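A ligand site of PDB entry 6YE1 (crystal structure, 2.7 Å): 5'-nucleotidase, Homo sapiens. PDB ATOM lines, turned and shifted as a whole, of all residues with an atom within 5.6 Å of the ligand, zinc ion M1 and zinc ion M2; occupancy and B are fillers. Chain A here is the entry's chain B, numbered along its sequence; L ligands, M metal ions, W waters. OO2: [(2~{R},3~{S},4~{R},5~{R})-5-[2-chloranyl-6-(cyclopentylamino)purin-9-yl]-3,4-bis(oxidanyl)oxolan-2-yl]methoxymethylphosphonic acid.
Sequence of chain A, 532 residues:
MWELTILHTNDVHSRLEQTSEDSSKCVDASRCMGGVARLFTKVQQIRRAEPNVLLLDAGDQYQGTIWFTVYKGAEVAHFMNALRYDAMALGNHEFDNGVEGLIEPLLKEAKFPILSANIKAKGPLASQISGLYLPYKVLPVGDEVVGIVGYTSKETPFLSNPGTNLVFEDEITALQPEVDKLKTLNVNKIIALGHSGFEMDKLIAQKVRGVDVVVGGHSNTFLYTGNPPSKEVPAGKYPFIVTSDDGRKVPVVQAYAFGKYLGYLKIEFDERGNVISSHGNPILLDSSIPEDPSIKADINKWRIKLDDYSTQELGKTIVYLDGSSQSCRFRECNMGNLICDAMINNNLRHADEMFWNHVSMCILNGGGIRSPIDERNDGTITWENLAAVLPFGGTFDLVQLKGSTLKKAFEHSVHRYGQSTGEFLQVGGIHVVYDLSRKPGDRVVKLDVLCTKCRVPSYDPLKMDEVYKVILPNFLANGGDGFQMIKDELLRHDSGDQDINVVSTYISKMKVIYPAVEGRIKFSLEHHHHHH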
ATOM      1  N   ASP A  11       1.305 -26.959  29.714  1.00  0.00           N
ATOM      2  CA  ASP A  11       0.502 -26.416  28.628  1.00  0.00           C
ATOM      3  C   ASP A  11       1.392 -26.088  27.404  1.00  0.00           C
ATOM      4  O   ASP A  11       1.276 -24.994  26.815  1.00  0.00           O
ATOM      5  CB  ASP A  11      -0.366 -25.215  29.085  1.00  0.00           C
ATOM      6  CG  ASP A  11      -1.213 -25.441  30.327  1.00  0.00           C
ATOM      7  OD1 ASP A  11      -0.657 -25.409  31.432  1.00  0.00           O
ATOM      8  OD2 ASP A  11      -2.456 -25.599  30.195  1.00  0.00           O
ATOM      9  N   HIS A  13       1.129 -27.382  24.584  1.00  0.00           N
ATOM     10  CA  HIS A  13       0.081 -27.271  23.569  1.00  0.00           C
ATOM     11  C   HIS A  13       0.596 -27.375  22.109  1.00  0.00           C
ATOM     12  O   HIS A  13       0.451 -26.431  21.321  1.00  0.00           O
ATOM     13  CB  HIS A  13      -0.757 -25.986  23.793  1.00  0.00           C
ATOM     14  CG  HIS A  13      -1.775 -26.117  24.896  1.00  0.00           C
ATOM     15  ND1 HIS A  13      -2.707 -27.149  24.915  1.00  0.00           N
ATOM     16  CD2 HIS A  13      -2.010 -25.312  25.963  1.00  0.00           C
ATOM     17  CE1 HIS A  13      -3.428 -26.952  25.996  1.00  0.00           C
ATOM     18  NE2 HIS A  13      -3.050 -25.861  26.664  1.00  0.00           N
ATOM     19  N   ASP A  60      -1.484 -30.961  29.313  1.00  0.00           N
ATOM     20  CA  ASP A  60      -1.853 -30.147  28.170  1.00  0.00           C
ATOM     21  C   ASP A  60      -0.713 -30.074  27.125  1.00  0.00           C
ATOM     22  O   ASP A  60      -0.354 -29.010  26.610  1.00  0.00           O
ATOM     23  CB  ASP A  60      -2.415 -28.756  28.536  1.00  0.00           C
ATOM     24  CG  ASP A  60      -3.903 -28.662  28.821  1.00  0.00           C
ATOM     25  OD1 ASP A  60      -4.558 -29.722  28.992  1.00  0.00           O
ATOM     26  OD2 ASP A  60      -4.403 -27.511  28.929  1.00  0.00           O
ATOM     27  N   GLN A  63      -3.212 -30.802  21.792  1.00  0.00           N
ATOM     28  CA  GLN A  63      -3.943 -29.694  21.136  1.00  0.00           C
ATOM     29  C   GLN A  63      -3.173 -28.361  21.011  1.00  0.00           C
ATOM     30  O   GLN A  63      -2.560 -27.906  21.979  1.00  0.00           O
ATOM     31  CB  GLN A  63      -5.318 -29.455  21.830  1.00  0.00           C
ATOM     32  CG  GLN A  63      -6.380 -28.843  20.924  1.00  0.00           C
ATOM     33  CD  GLN A  63      -6.881 -29.810  19.897  1.00  0.00           C
ATOM     34  OE1 GLN A  63      -6.410 -29.830  18.756  1.00  0.00           O
ATOM     35  NE2 GLN A  63      -7.840 -30.646  20.277  1.00  0.00           N
ATOM     36  N   GLY A  91      -3.703 -33.606  31.765  1.00  0.00           N
ATOM     37  CA  GLY A  91      -4.344 -32.329  31.497  1.00  0.00           C
ATOM     38  C   GLY A  91      -5.663 -32.625  30.819  1.00  0.00           C
ATOM     39  O   GLY A  91      -5.874 -33.753  30.347  1.00  0.00           O
ATOM     40  N   ASN A  92      -6.561 -31.612  30.769  1.00  0.00           N
ATOM     41  CA  ASN A  92      -7.887 -31.730  30.183  1.00  0.00           C
ATOM     42  C   ASN A  92      -7.865 -32.039  28.693  1.00  0.00           C
ATOM     43  O   ASN A  92      -8.651 -32.858  28.220  1.00  0.00           O
ATOM     44  CB  ASN A  92      -8.746 -30.505  30.498  1.00  0.00           C
ATOM     45  CG  ASN A  92      -8.202 -29.189  29.996  1.00  0.00           C
ATOM     46  OD1 ASN A  92      -7.134 -28.730  30.421  1.00  0.00           O
ATOM     47  ND2 ASN A  92      -8.957 -28.554  29.112  1.00  0.00           N
ATOM     48  N   HIS A  93      -6.892 -31.458  27.972  1.00  0.00           N
ATOM     49  CA  HIS A  93      -6.745 -31.628  26.528  1.00  0.00           C
ATOM     50  C   HIS A  93      -6.279 -33.013  26.104  1.00  0.00           C
ATOM     51  O   HIS A  93      -6.490 -33.388  24.953  1.00  0.00           O
ATOM     52  CB  HIS A  93      -5.862 -30.507  25.937  1.00  0.00           C
ATOM     53  CG  HIS A  93      -6.572 -29.193  26.001  1.00  0.00           C
ATOM     54  ND1 HIS A  93      -7.493 -28.822  25.043  1.00  0.00           N
ATOM     55  CD2 HIS A  93      -6.602 -28.275  27.003  1.00  0.00           C
ATOM     56  CE1 HIS A  93      -7.999 -27.679  25.452  1.00  0.00           C
ATOM     57  NE2 HIS A  93      -7.482 -27.315  26.622  1.00  0.00           N
ATOM     58  N   ASP A  96      -9.217 -34.643  24.537  1.00  0.00           N
ATOM     59  CA  ASP A  96      -9.827 -33.975  23.377  1.00  0.00           C
ATOM     60  C   ASP A  96     -10.170 -34.930  22.254  1.00  0.00           C
ATOM     61  O   ASP A  96     -11.187 -34.721  21.589  1.00  0.00           O
ATOM     62  CB  ASP A  96      -8.913 -32.876  22.840  1.00  0.00           C
ATOM     63  CG  ASP A  96      -8.899 -31.560  23.587  1.00  0.00           C
ATOM     64  OD1 ASP A  96      -9.612 -31.440  24.621  1.00  0.00           O
ATOM     65  OD2 ASP A  96      -8.174 -30.647  23.163  1.00  0.00           O
ATOM     66  N   LEU A 159     -14.919 -29.257  29.270  1.00  0.00           N
ATOM     67  CA  LEU A 159     -13.858 -28.631  28.479  1.00  0.00           C
ATOM     68  C   LEU A 159     -13.350 -29.541  27.374  1.00  0.00           C
ATOM     69  O   LEU A 159     -12.814 -29.053  26.377  1.00  0.00           O
ATOM     70  CB  LEU A 159     -12.692 -28.237  29.388  1.00  0.00           C
ATOM     71  CG  LEU A 159     -12.878 -26.983  30.217  1.00  0.00           C
ATOM     72  CD1 LEU A 159     -11.758 -26.809  31.203  1.00  0.00           C
ATOM     73  CD2 LEU A 159     -12.946 -25.761  29.347  1.00  0.00           C
ATOM     74  N   SER A 160     -13.495 -30.870  27.558  1.00  0.00           N
ATOM     75  CA  SER A 160     -13.010 -31.907  26.643  1.00  0.00           C
ATOM     76  C   SER A 160     -14.010 -33.070  26.515  1.00  0.00           C
ATOM     77  O   SER A 160     -15.140 -32.962  26.990  1.00  0.00           O
ATOM     78  CB  SER A 160     -11.656 -32.419  27.141  1.00  0.00           C
ATOM     79  OG  SER A 160     -10.993 -33.173  26.149  1.00  0.00           O
ATOM     80  N   ASN A 161     -13.583 -34.192  25.866  1.00  0.00           N
ATOM     81  CA  ASN A 161     -14.370 -35.411  25.611  1.00  0.00           C
ATOM     82  C   ASN A 161     -13.830 -36.627  26.402  1.00  0.00           C
ATOM     83  O   ASN A 161     -13.377 -37.575  25.760  1.00  0.00           O
ATOM     84  CB  ASN A 161     -14.372 -35.747  24.097  1.00  0.00           C
ATOM     85  CG  ASN A 161     -14.703 -34.618  23.126  1.00  0.00           C
ATOM     86  OD1 ASN A 161     -15.446 -33.671  23.430  1.00  0.00           O
ATOM     87  ND2 ASN A 161     -14.182 -34.713  21.910  1.00  0.00           N
ATOM     88  N   HIS A 195      -3.028 -30.563  36.733  1.00  0.00           N
ATOM     89  CA  HIS A 195      -3.637 -29.652  35.782  1.00  0.00           C
ATOM     90  C   HIS A 195      -4.998 -29.114  36.213  1.00  0.00           C
ATOM     91  O   HIS A 195      -6.024 -29.500  35.670  1.00  0.00           O
ATOM     92  CB  HIS A 195      -3.763 -30.390  34.451  1.00  0.00           C
ATOM     93  CG  HIS A 195      -3.794 -29.452  33.298  1.00  0.00           C
ATOM     94  ND1 HIS A 195      -2.625 -28.931  32.769  1.00  0.00           N
ATOM     95  CD2 HIS A 195      -4.850 -28.958  32.619  1.00  0.00           C
ATOM     96  CE1 HIS A 195      -3.017 -28.131  31.796  1.00  0.00           C
ATOM     97  NE2 HIS A 195      -4.342 -28.108  31.670  1.00  0.00           N
ATOM     98  N   HIS A 218      -2.422 -25.413  33.559  1.00  0.00           N
ATOM     99  CA  HIS A 218      -3.829 -25.148  33.176  1.00  0.00           C
ATOM    100  C   HIS A 218      -4.150 -23.659  33.032  1.00  0.00           C
ATOM    101  O   HIS A 218      -4.621 -23.227  31.970  1.00  0.00           O
ATOM    102  CB  HIS A 218      -4.833 -25.855  34.098  1.00  0.00           C
ATOM    103  CG  HIS A 218      -6.245 -25.811  33.599  1.00  0.00           C
ATOM    104  ND1 HIS A 218      -6.685 -26.652  32.578  1.00  0.00           N
ATOM    105  CD2 HIS A 218      -7.270 -25.024  33.981  1.00  0.00           C
ATOM    106  CE1 HIS A 218      -7.958 -26.372  32.413  1.00  0.00           C
ATOM    107  NE2 HIS A 218      -8.348 -25.367  33.212  1.00  0.00           N
ATOM    108  N   SER A 219      -3.887 -22.889  34.097  1.00  0.00           N
ATOM    109  CA  SER A 219      -4.095 -21.444  34.166  1.00  0.00           C
ATOM    110  C   SER A 219      -2.993 -20.588  33.458  1.00  0.00           C
ATOM    111  O   SER A 219      -3.025 -19.358  33.584  1.00  0.00           O
ATOM    112  CB  SER A 219      -4.225 -21.033  35.633  1.00  0.00           C
ATOM    113  OG  SER A 219      -3.103 -21.470  36.386  1.00  0.00           O
ATOM    114  N   ASN A 220      -2.036 -21.235  32.730  1.00  0.00           N
ATOM    115  CA  ASN A 220      -0.912 -20.599  32.016  1.00  0.00           C
ATOM    116  C   ASN A 220      -0.312 -19.477  32.839  1.00  0.00           C
ATOM    117  O   ASN A 220      -0.242 -18.323  32.403  1.00  0.00           O
ATOM    118  CB  ASN A 220      -1.352 -20.112  30.643  1.00  0.00           C
ATOM    119  CG  ASN A 220      -1.691 -21.177  29.659  1.00  0.00           C
ATOM    120  OD1 ASN A 220      -2.078 -22.318  29.990  1.00  0.00           O
ATOM    121  ND2 ASN A 220      -1.557 -20.823  28.393  1.00  0.00           N
ATOM    122  N   ARG A 329      -8.798 -12.373  26.444  1.00  0.00           N
ATOM    123  CA  ARG A 329      -9.532 -12.805  27.630  1.00  0.00           C
ATOM    124  C   ARG A 329      -9.735 -11.692  28.623  1.00  0.00           C
ATOM    125  O   ARG A 329     -10.378 -11.909  29.649  1.00  0.00           O
ATOM    126  CB  ARG A 329      -8.880 -14.024  28.302  1.00  0.00           C
ATOM    127  CG  ARG A 329      -8.669 -15.236  27.394  1.00  0.00           C
ATOM    128  CD  ARG A 329      -8.251 -16.430  28.219  1.00  0.00           C
ATOM    129  NE  ARG A 329      -7.785 -17.548  27.386  1.00  0.00           N
ATOM    130  CZ  ARG A 329      -7.708 -18.806  27.794  1.00  0.00           C
ATOM    131  NH1 ARG A 329      -8.088 -19.148  29.029  1.00  0.00           N
ATOM    132  NH2 ARG A 329      -7.280 -19.755  26.958  1.00  0.00           N
ATOM    133  N   ASN A 365     -16.321 -17.078  23.120  1.00  0.00           N
ATOM    134  CA  ASN A 365     -15.476 -17.218  24.302  1.00  0.00           C
ATOM    135  C   ASN A 365     -13.999 -17.023  23.875  1.00  0.00           C
ATOM    136  O   ASN A 365     -13.503 -17.737  22.993  1.00  0.00           O
ATOM    137  CB  ASN A 365     -15.662 -18.600  24.912  1.00  0.00           C
ATOM    138  CG  ASN A 365     -15.346 -19.747  23.961  1.00  0.00           C
ATOM    139  OD1 ASN A 365     -15.928 -19.861  22.864  1.00  0.00           O
ATOM    140  ND2 ASN A 365     -14.394 -20.602  24.329  1.00  0.00           N
ATOM    141  N   GLY A 366     -13.353 -16.035  24.491  1.00  0.00           N
ATOM    142  CA  GLY A 366     -11.961 -15.640  24.259  1.00  0.00           C
ATOM    143  C   GLY A 366     -10.938 -16.751  24.416  1.00  0.00           C
ATOM    144  O   GLY A 366      -9.928 -16.780  23.704  1.00  0.00           O
ATOM    145  N   GLY A 367     -11.209 -17.676  25.326  1.00  0.00           N
ATOM    146  CA  GLY A 367     -10.377 -18.843  25.563  1.00  0.00           C
ATOM    147  C   GLY A 367     -10.322 -19.792  24.371  1.00  0.00           C
ATOM    148  O   GLY A 367      -9.402 -20.596  24.276  1.00  0.00           O
ATOM    149  N   GLY A 368     -11.311 -19.680  23.487  1.00  0.00           N
ATOM    150  CA  GLY A 368     -11.418 -20.474  22.265  1.00  0.00           C
ATOM    151  C   GLY A 368     -10.448 -20.009  21.199  1.00  0.00           C
ATOM    152  O   GLY A 368     -10.214 -20.730  20.222  1.00  0.00           O
ATOM    153  N   ARG A 370      -6.953 -19.611  20.385  1.00  0.00           N
ATOM    154  CA  ARG A 370      -5.800 -20.335  20.878  1.00  0.00           C
ATOM    155  C   ARG A 370      -4.410 -19.869  20.354  1.00  0.00           C
ATOM    156  O   ARG A 370      -3.407 -20.353  20.910  1.00  0.00           O
ATOM    157  CB  ARG A 370      -6.000 -21.845  20.675  1.00  0.00           C
ATOM    158  CG  ARG A 370      -7.089 -22.470  21.602  1.00  0.00           C
ATOM    159  CD  ARG A 370      -6.923 -22.106  23.095  1.00  0.00           C
ATOM    160  NE  ARG A 370      -7.123 -23.241  24.015  1.00  0.00           N
ATOM    161  CZ  ARG A 370      -6.126 -23.898  24.639  1.00  0.00           C
ATOM    162  NH1 ARG A 370      -6.397 -24.935  25.426  1.00  0.00           N
ATOM    163  NH2 ARG A 370      -4.866 -23.525  24.477  1.00  0.00           N
ATOM    164  N   PHE A 392      -9.340 -26.885  17.764  1.00  0.00           N
ATOM    165  CA  PHE A 392     -10.438 -27.651  18.300  1.00  0.00           C
ATOM    166  C   PHE A 392     -11.192 -28.495  17.292  1.00  0.00           C
ATOM    167  O   PHE A 392     -11.142 -29.712  17.421  1.00  0.00           O
ATOM    168  CB  PHE A 392     -11.359 -26.738  19.100  1.00  0.00           C
ATOM    169  CG  PHE A 392     -10.652 -26.262  20.344  1.00  0.00           C
ATOM    170  CD1 PHE A 392      -9.822 -27.117  21.080  1.00  0.00           C
ATOM    171  CD2 PHE A 392     -10.811 -24.966  20.810  1.00  0.00           C
ATOM    172  CE1 PHE A 392      -9.160 -26.667  22.225  1.00  0.00           C
ATOM    173  CE2 PHE A 392     -10.166 -24.522  21.967  1.00  0.00           C
ATOM    174  CZ  PHE A 392      -9.351 -25.386  22.670  1.00  0.00           C
ATOM    175  N   GLY A 393     -11.817 -27.904  16.294  1.00  0.00           N
ATOM    176  CA  GLY A 393     -12.579 -28.679  15.302  1.00  0.00           C
ATOM    177  C   GLY A 393     -14.088 -28.575  15.483  1.00  0.00           C
ATOM    178  O   GLY A 393     -14.843 -29.448  15.024  1.00  0.00           O
ATOM    179  N   THR A 421      -9.512 -16.185  32.660  1.00  0.00           N
ATOM    180  CA  THR A 421     -10.648 -17.065  32.430  1.00  0.00           C
ATOM    181  C   THR A 421     -11.173 -16.823  31.010  1.00  0.00           C
ATOM    182  O   THR A 421     -11.425 -15.680  30.627  1.00  0.00           O
ATOM    183  CB  THR A 421     -11.688 -16.908  33.544  1.00  0.00           C
ATOM    184  OG1 THR A 421     -11.818 -15.521  33.889  1.00  0.00           O
ATOM    185  CG2 THR A 421     -11.311 -17.713  34.790  1.00  0.00           C
ATOM    186  N   GLY A 422     -11.223 -17.898  30.229  1.00  0.00           N
ATOM    187  CA  GLY A 422     -11.643 -17.907  28.828  1.00  0.00           C
ATOM    188  C   GLY A 422     -13.125 -17.747  28.542  1.00  0.00           C
ATOM    189  O   GLY A 422     -13.525 -17.823  27.374  1.00  0.00           O
ATOM    190  N   GLU A 423     -13.968 -17.534  29.590  1.00  0.00           N
ATOM    191  CA  GLU A 423     -15.403 -17.319  29.397  1.00  0.00           C
ATOM    192  C   GLU A 423     -15.688 -15.960  28.723  1.00  0.00           C
ATOM    193  O   GLU A 423     -16.656 -15.858  27.943  1.00  0.00           O
ATOM    194  CB  GLU A 423     -16.197 -17.510  30.699  1.00  0.00           C
ATOM    195  CG  GLU A 423     -16.254 -16.308  31.631  1.00  0.00           C
ATOM    196  CD  GLU A 423     -15.530 -16.445  32.942  1.00  0.00           C
ATOM    197  OE1 GLU A 423     -15.571 -15.494  33.756  1.00  0.00           O
ATOM    198  OE2 GLU A 423     -14.902 -17.498  33.166  1.00  0.00           O
ATOM    199  N   PRO A 473     -19.849 -20.371  18.820  1.00  0.00           N
ATOM    200  CA  PRO A 473     -19.269 -21.720  18.646  1.00  0.00           C
ATOM    201  C   PRO A 473     -20.136 -22.792  19.341  1.00  0.00           C
ATOM    202  O   PRO A 473     -20.789 -22.521  20.354  1.00  0.00           O
ATOM    203  CB  PRO A 473     -17.876 -21.594  19.263  1.00  0.00           C
ATOM    204  CG  PRO A 473     -18.019 -20.523  20.270  1.00  0.00           C
ATOM    205  CD  PRO A 473     -19.054 -19.552  19.769  1.00  0.00           C
ATOM    206  N   PHE A 475     -19.330 -25.168  21.204  1.00  0.00           N
ATOM    207  CA  PHE A 475     -18.846 -25.280  22.596  1.00  0.00           C
ATOM    208  C   PHE A 475     -19.733 -24.475  23.561  1.00  0.00           C
ATOM    209  O   PHE A 475     -20.129 -24.998  24.607  1.00  0.00           O
ATOM    210  CB  PHE A 475     -17.384 -24.815  22.690  1.00  0.00           C
ATOM    211  CG  PHE A 475     -16.794 -24.727  24.088  1.00  0.00           C
ATOM    212  CD1 PHE A 475     -16.511 -25.880  24.804  1.00  0.00           C
ATOM    213  CD2 PHE A 475     -16.473 -23.497  24.638  1.00  0.00           C
ATOM    214  CE1 PHE A 475     -15.966 -25.792  26.075  1.00  0.00           C
ATOM    215  CE2 PHE A 475     -15.923 -23.415  25.913  1.00  0.00           C
ATOM    216  CZ  PHE A 475     -15.644 -24.567  26.616  1.00  0.00           C
ATOM    217  N   ASP A 481     -18.099 -23.291  28.985  1.00  0.00           N
ATOM    218  CA  ASP A 481     -17.597 -22.112  29.695  1.00  0.00           C
ATOM    219  C   ASP A 481     -18.606 -21.547  30.723  1.00  0.00           C
ATOM    220  O   ASP A 481     -18.584 -20.357  31.038  1.00  0.00           O
ATOM    221  CB  ASP A 481     -17.075 -21.034  28.717  1.00  0.00           C
ATOM    222  CG  ASP A 481     -15.585 -20.905  28.593  1.00  0.00           C
ATOM    223  OD1 ASP A 481     -14.856 -21.502  29.437  1.00  0.00           O
ATOM    224  OD2 ASP A 481     -15.138 -20.202  27.674  1.00  0.00           O
HETATM  225  C1  OO2 L   1     -13.501 -24.358  23.099  1.00  0.00           C
HETATM  226  C2  OO2 L   1     -12.217 -24.468  24.880  1.00  0.00           C
HETATM  227  N1  OO2 L   1     -13.456 -25.657  22.827  1.00  0.00           N
HETATM  228  N2  OO2 L   1     -12.967 -23.667  24.099  1.00  0.00           N
HETATM  229  C3  OO2 L   1     -12.706 -26.426  23.649  1.00  0.00           C
HETATM  230  O1  OO2 L   1     -12.023 -21.159  29.596  1.00  0.00           O
HETATM  231  C4  OO2 L   1     -11.572 -22.220  28.773  1.00  0.00           C
HETATM  232  C5  OO2 L   1     -12.301 -22.276  27.423  1.00  0.00           C
HETATM  233  O2  OO2 L   1     -12.692 -20.978  27.002  1.00  0.00           O
HETATM  234  C6  OO2 L   1     -10.125 -21.962  28.361  1.00  0.00           C
HETATM  235  C7  OO2 L   1      -9.102 -22.380  29.379  1.00  0.00           C
HETATM  236  O3  OO2 L   1      -7.802 -22.278  28.785  1.00  0.00           O
HETATM  237  C8  OO2 L   1      -6.854 -23.126  29.408  1.00  0.00           C
HETATM  238  P1  OO2 L   1      -6.830 -24.819  28.802  1.00  0.00           P
HETATM  239  O4  OO2 L   1      -6.850 -25.822  29.914  1.00  0.00           O
HETATM  240  O5  OO2 L   1      -5.534 -24.848  27.967  1.00  0.00           O
HETATM  241  O6  OO2 L   1      -8.009 -25.059  27.844  1.00  0.00           O
HETATM  242  O7  OO2 L   1      -9.969 -22.700  27.133  1.00  0.00           O
HETATM  243  C9  OO2 L   1     -11.217 -22.749  26.461  1.00  0.00           C
HETATM  244  N3  OO2 L   1     -11.404 -24.085  25.918  1.00  0.00           N
HETATM  245  C10 OO2 L   1     -10.783 -25.235  26.330  1.00  0.00           C
HETATM  246  N4  OO2 L   1     -11.114 -26.309  25.648  1.00  0.00           N
HETATM  247  C11 OO2 L   1     -12.033 -25.825  24.730  1.00  0.00           C
HETATM  248 CL1  OO2 L   1     -14.253 -23.369  21.872  1.00  0.00          CL
HETATM  249  N5  OO2 L   1     -12.635 -27.758  23.426  1.00  0.00           N
HETATM  250  C12 OO2 L   1     -13.612 -28.589  22.723  1.00  0.00           C
HETATM  251  C13 OO2 L   1     -13.108 -29.038  21.362  1.00  0.00           C
HETATM  252  C14 OO2 L   1     -12.238 -30.256  21.649  1.00  0.00           C
HETATM  253  C15 OO2 L   1     -12.689 -30.774  22.989  1.00  0.00           C
HETATM  254  C16 OO2 L   1     -13.858 -29.896  23.418  1.00  0.00           C
HETATM  255 ZN    ZN M   1      -3.520 -25.188  28.653  1.00  0.00          ZN
HETATM  256 ZN    ZN M   2      -5.578 -26.984  30.635  1.00  0.00          ZN
HETATM  257  O   HOH W   1     -15.873 -27.085  21.048  1.00  0.00           O
HETATM  258  O   HOH W   2     -13.831 -20.899  19.998  1.00  0.00           O
HETATM  259  O   HOH W   3     -12.224 -32.400  19.170  1.00  0.00           O
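OD2 of Asp 481 sits at hydrogen-bond distance from O2 of the ligand, 2.7 Å away. O of Leu 159 lies within hydrogen-bond range of N5 of the ligand. The backbone NH (N) of Gly 422 lies close to an oxygen (O1) of the ligand (3.4 Å). O6 of the ligand is in salt-bridge range of NH1 of Arg 370, at 2.9 Å. O of Gly 422 sits at hydrogen-bond distance from O2 of the ligand, 3.3 Å away. NE2 of His 93 sits at hydrogen-bond distance from O6 of the ligand, at 2.6 Å. The side-chain amide nitrogen (ND2) of Asn 365 lies within hydrogen-bond range of an oxygen (O2) of the ligand, at 3.2 Å. NH1 of Arg 329 is in hydrogen-bond range of O3 of the ligand, at 3.2 Å.
Zinc ion M2 is bound by an oxygen (O4) of the ligand (1.9 Å), a ring nitrogen (NE2) of His 195 (2.0 Å), the side-chain carboxylate of Asp 60 (2.1 Å), a ring nitrogen (ND1) of His 218 (2.3 Å) and the side-chain amide oxygen of Asn 92 (2.3 Å). Zinc ion M2 has five donor atoms within binding distance.
Merely in contact with zinc ion M2: His 93. Within 4 Å of zinc ion M2: Asp 11, Asp 60, Asn 92, His 93, His 195 and His 218. The nearest printed residue that does not touch zinc ion M2 is His 13 (4.8 Å).
Merely in contact with zinc ion M1: Asn 220 (3.5 Å). Of the 29 residues printed, 4 come within 4 Å of zinc ion M1.
Zinc ion M1 is bound by the side-chain carboxylate of Asp 11 (1.9 Å), a ring nitrogen (NE2) of His 13 (2.2 Å), an oxygen (O5) of the ligand (2.2 Å) and the side-chain carboxylate of Asp 60 (2.5 Å).
The backbone NH (N) of His 218 lies within hydrogen-bond range of the side-chain carboxylate (OD1) of Asp 11, 2.8 Å away. The backbone carbonyl oxygen (O) of Gly 422 is in hydrogen-bond range of the backbone NH (N) of Gly 367 (3.1 Å). A ring nitrogen (NE2) of His 93 is in hydrogen-bond range of the guanidinium group (NH1) of Arg 370, 2.9 Å away. OG of Ser 160 is in hydrogen-bond range of O of Asn 92 (3.1 Å). OD2 of Asp 481 sits close to N of Glu 423 (3.5 Å). The backbone carbonyl oxygen of Gln 63 is in hydrogen-bond range of a ring nitrogen (ND1) of His 13, 3.0 Å away. OG of Ser 160 lies within hydrogen-bond range of OD1 of Asp 96. OD1 of Asn 220 lies close to OD2 of Asp 11 (3.3 Å).
Merely in contact with the ligand: Asp 96 (3.5 Å), Ser 160 (3.8 Å), Gly 367 (3.5 Å), Gly 368 (3.99 Å), Phe 392 (3.4 Å) and Phe 475 (3.5 Å). Hydrophobic or aromatic side chains that line the ligand: His 13, His 93, Leu 159, His 218, Phe 392 and Phe 475. Of the 29 residues printed, 19 come within 4 Å of the ligand.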
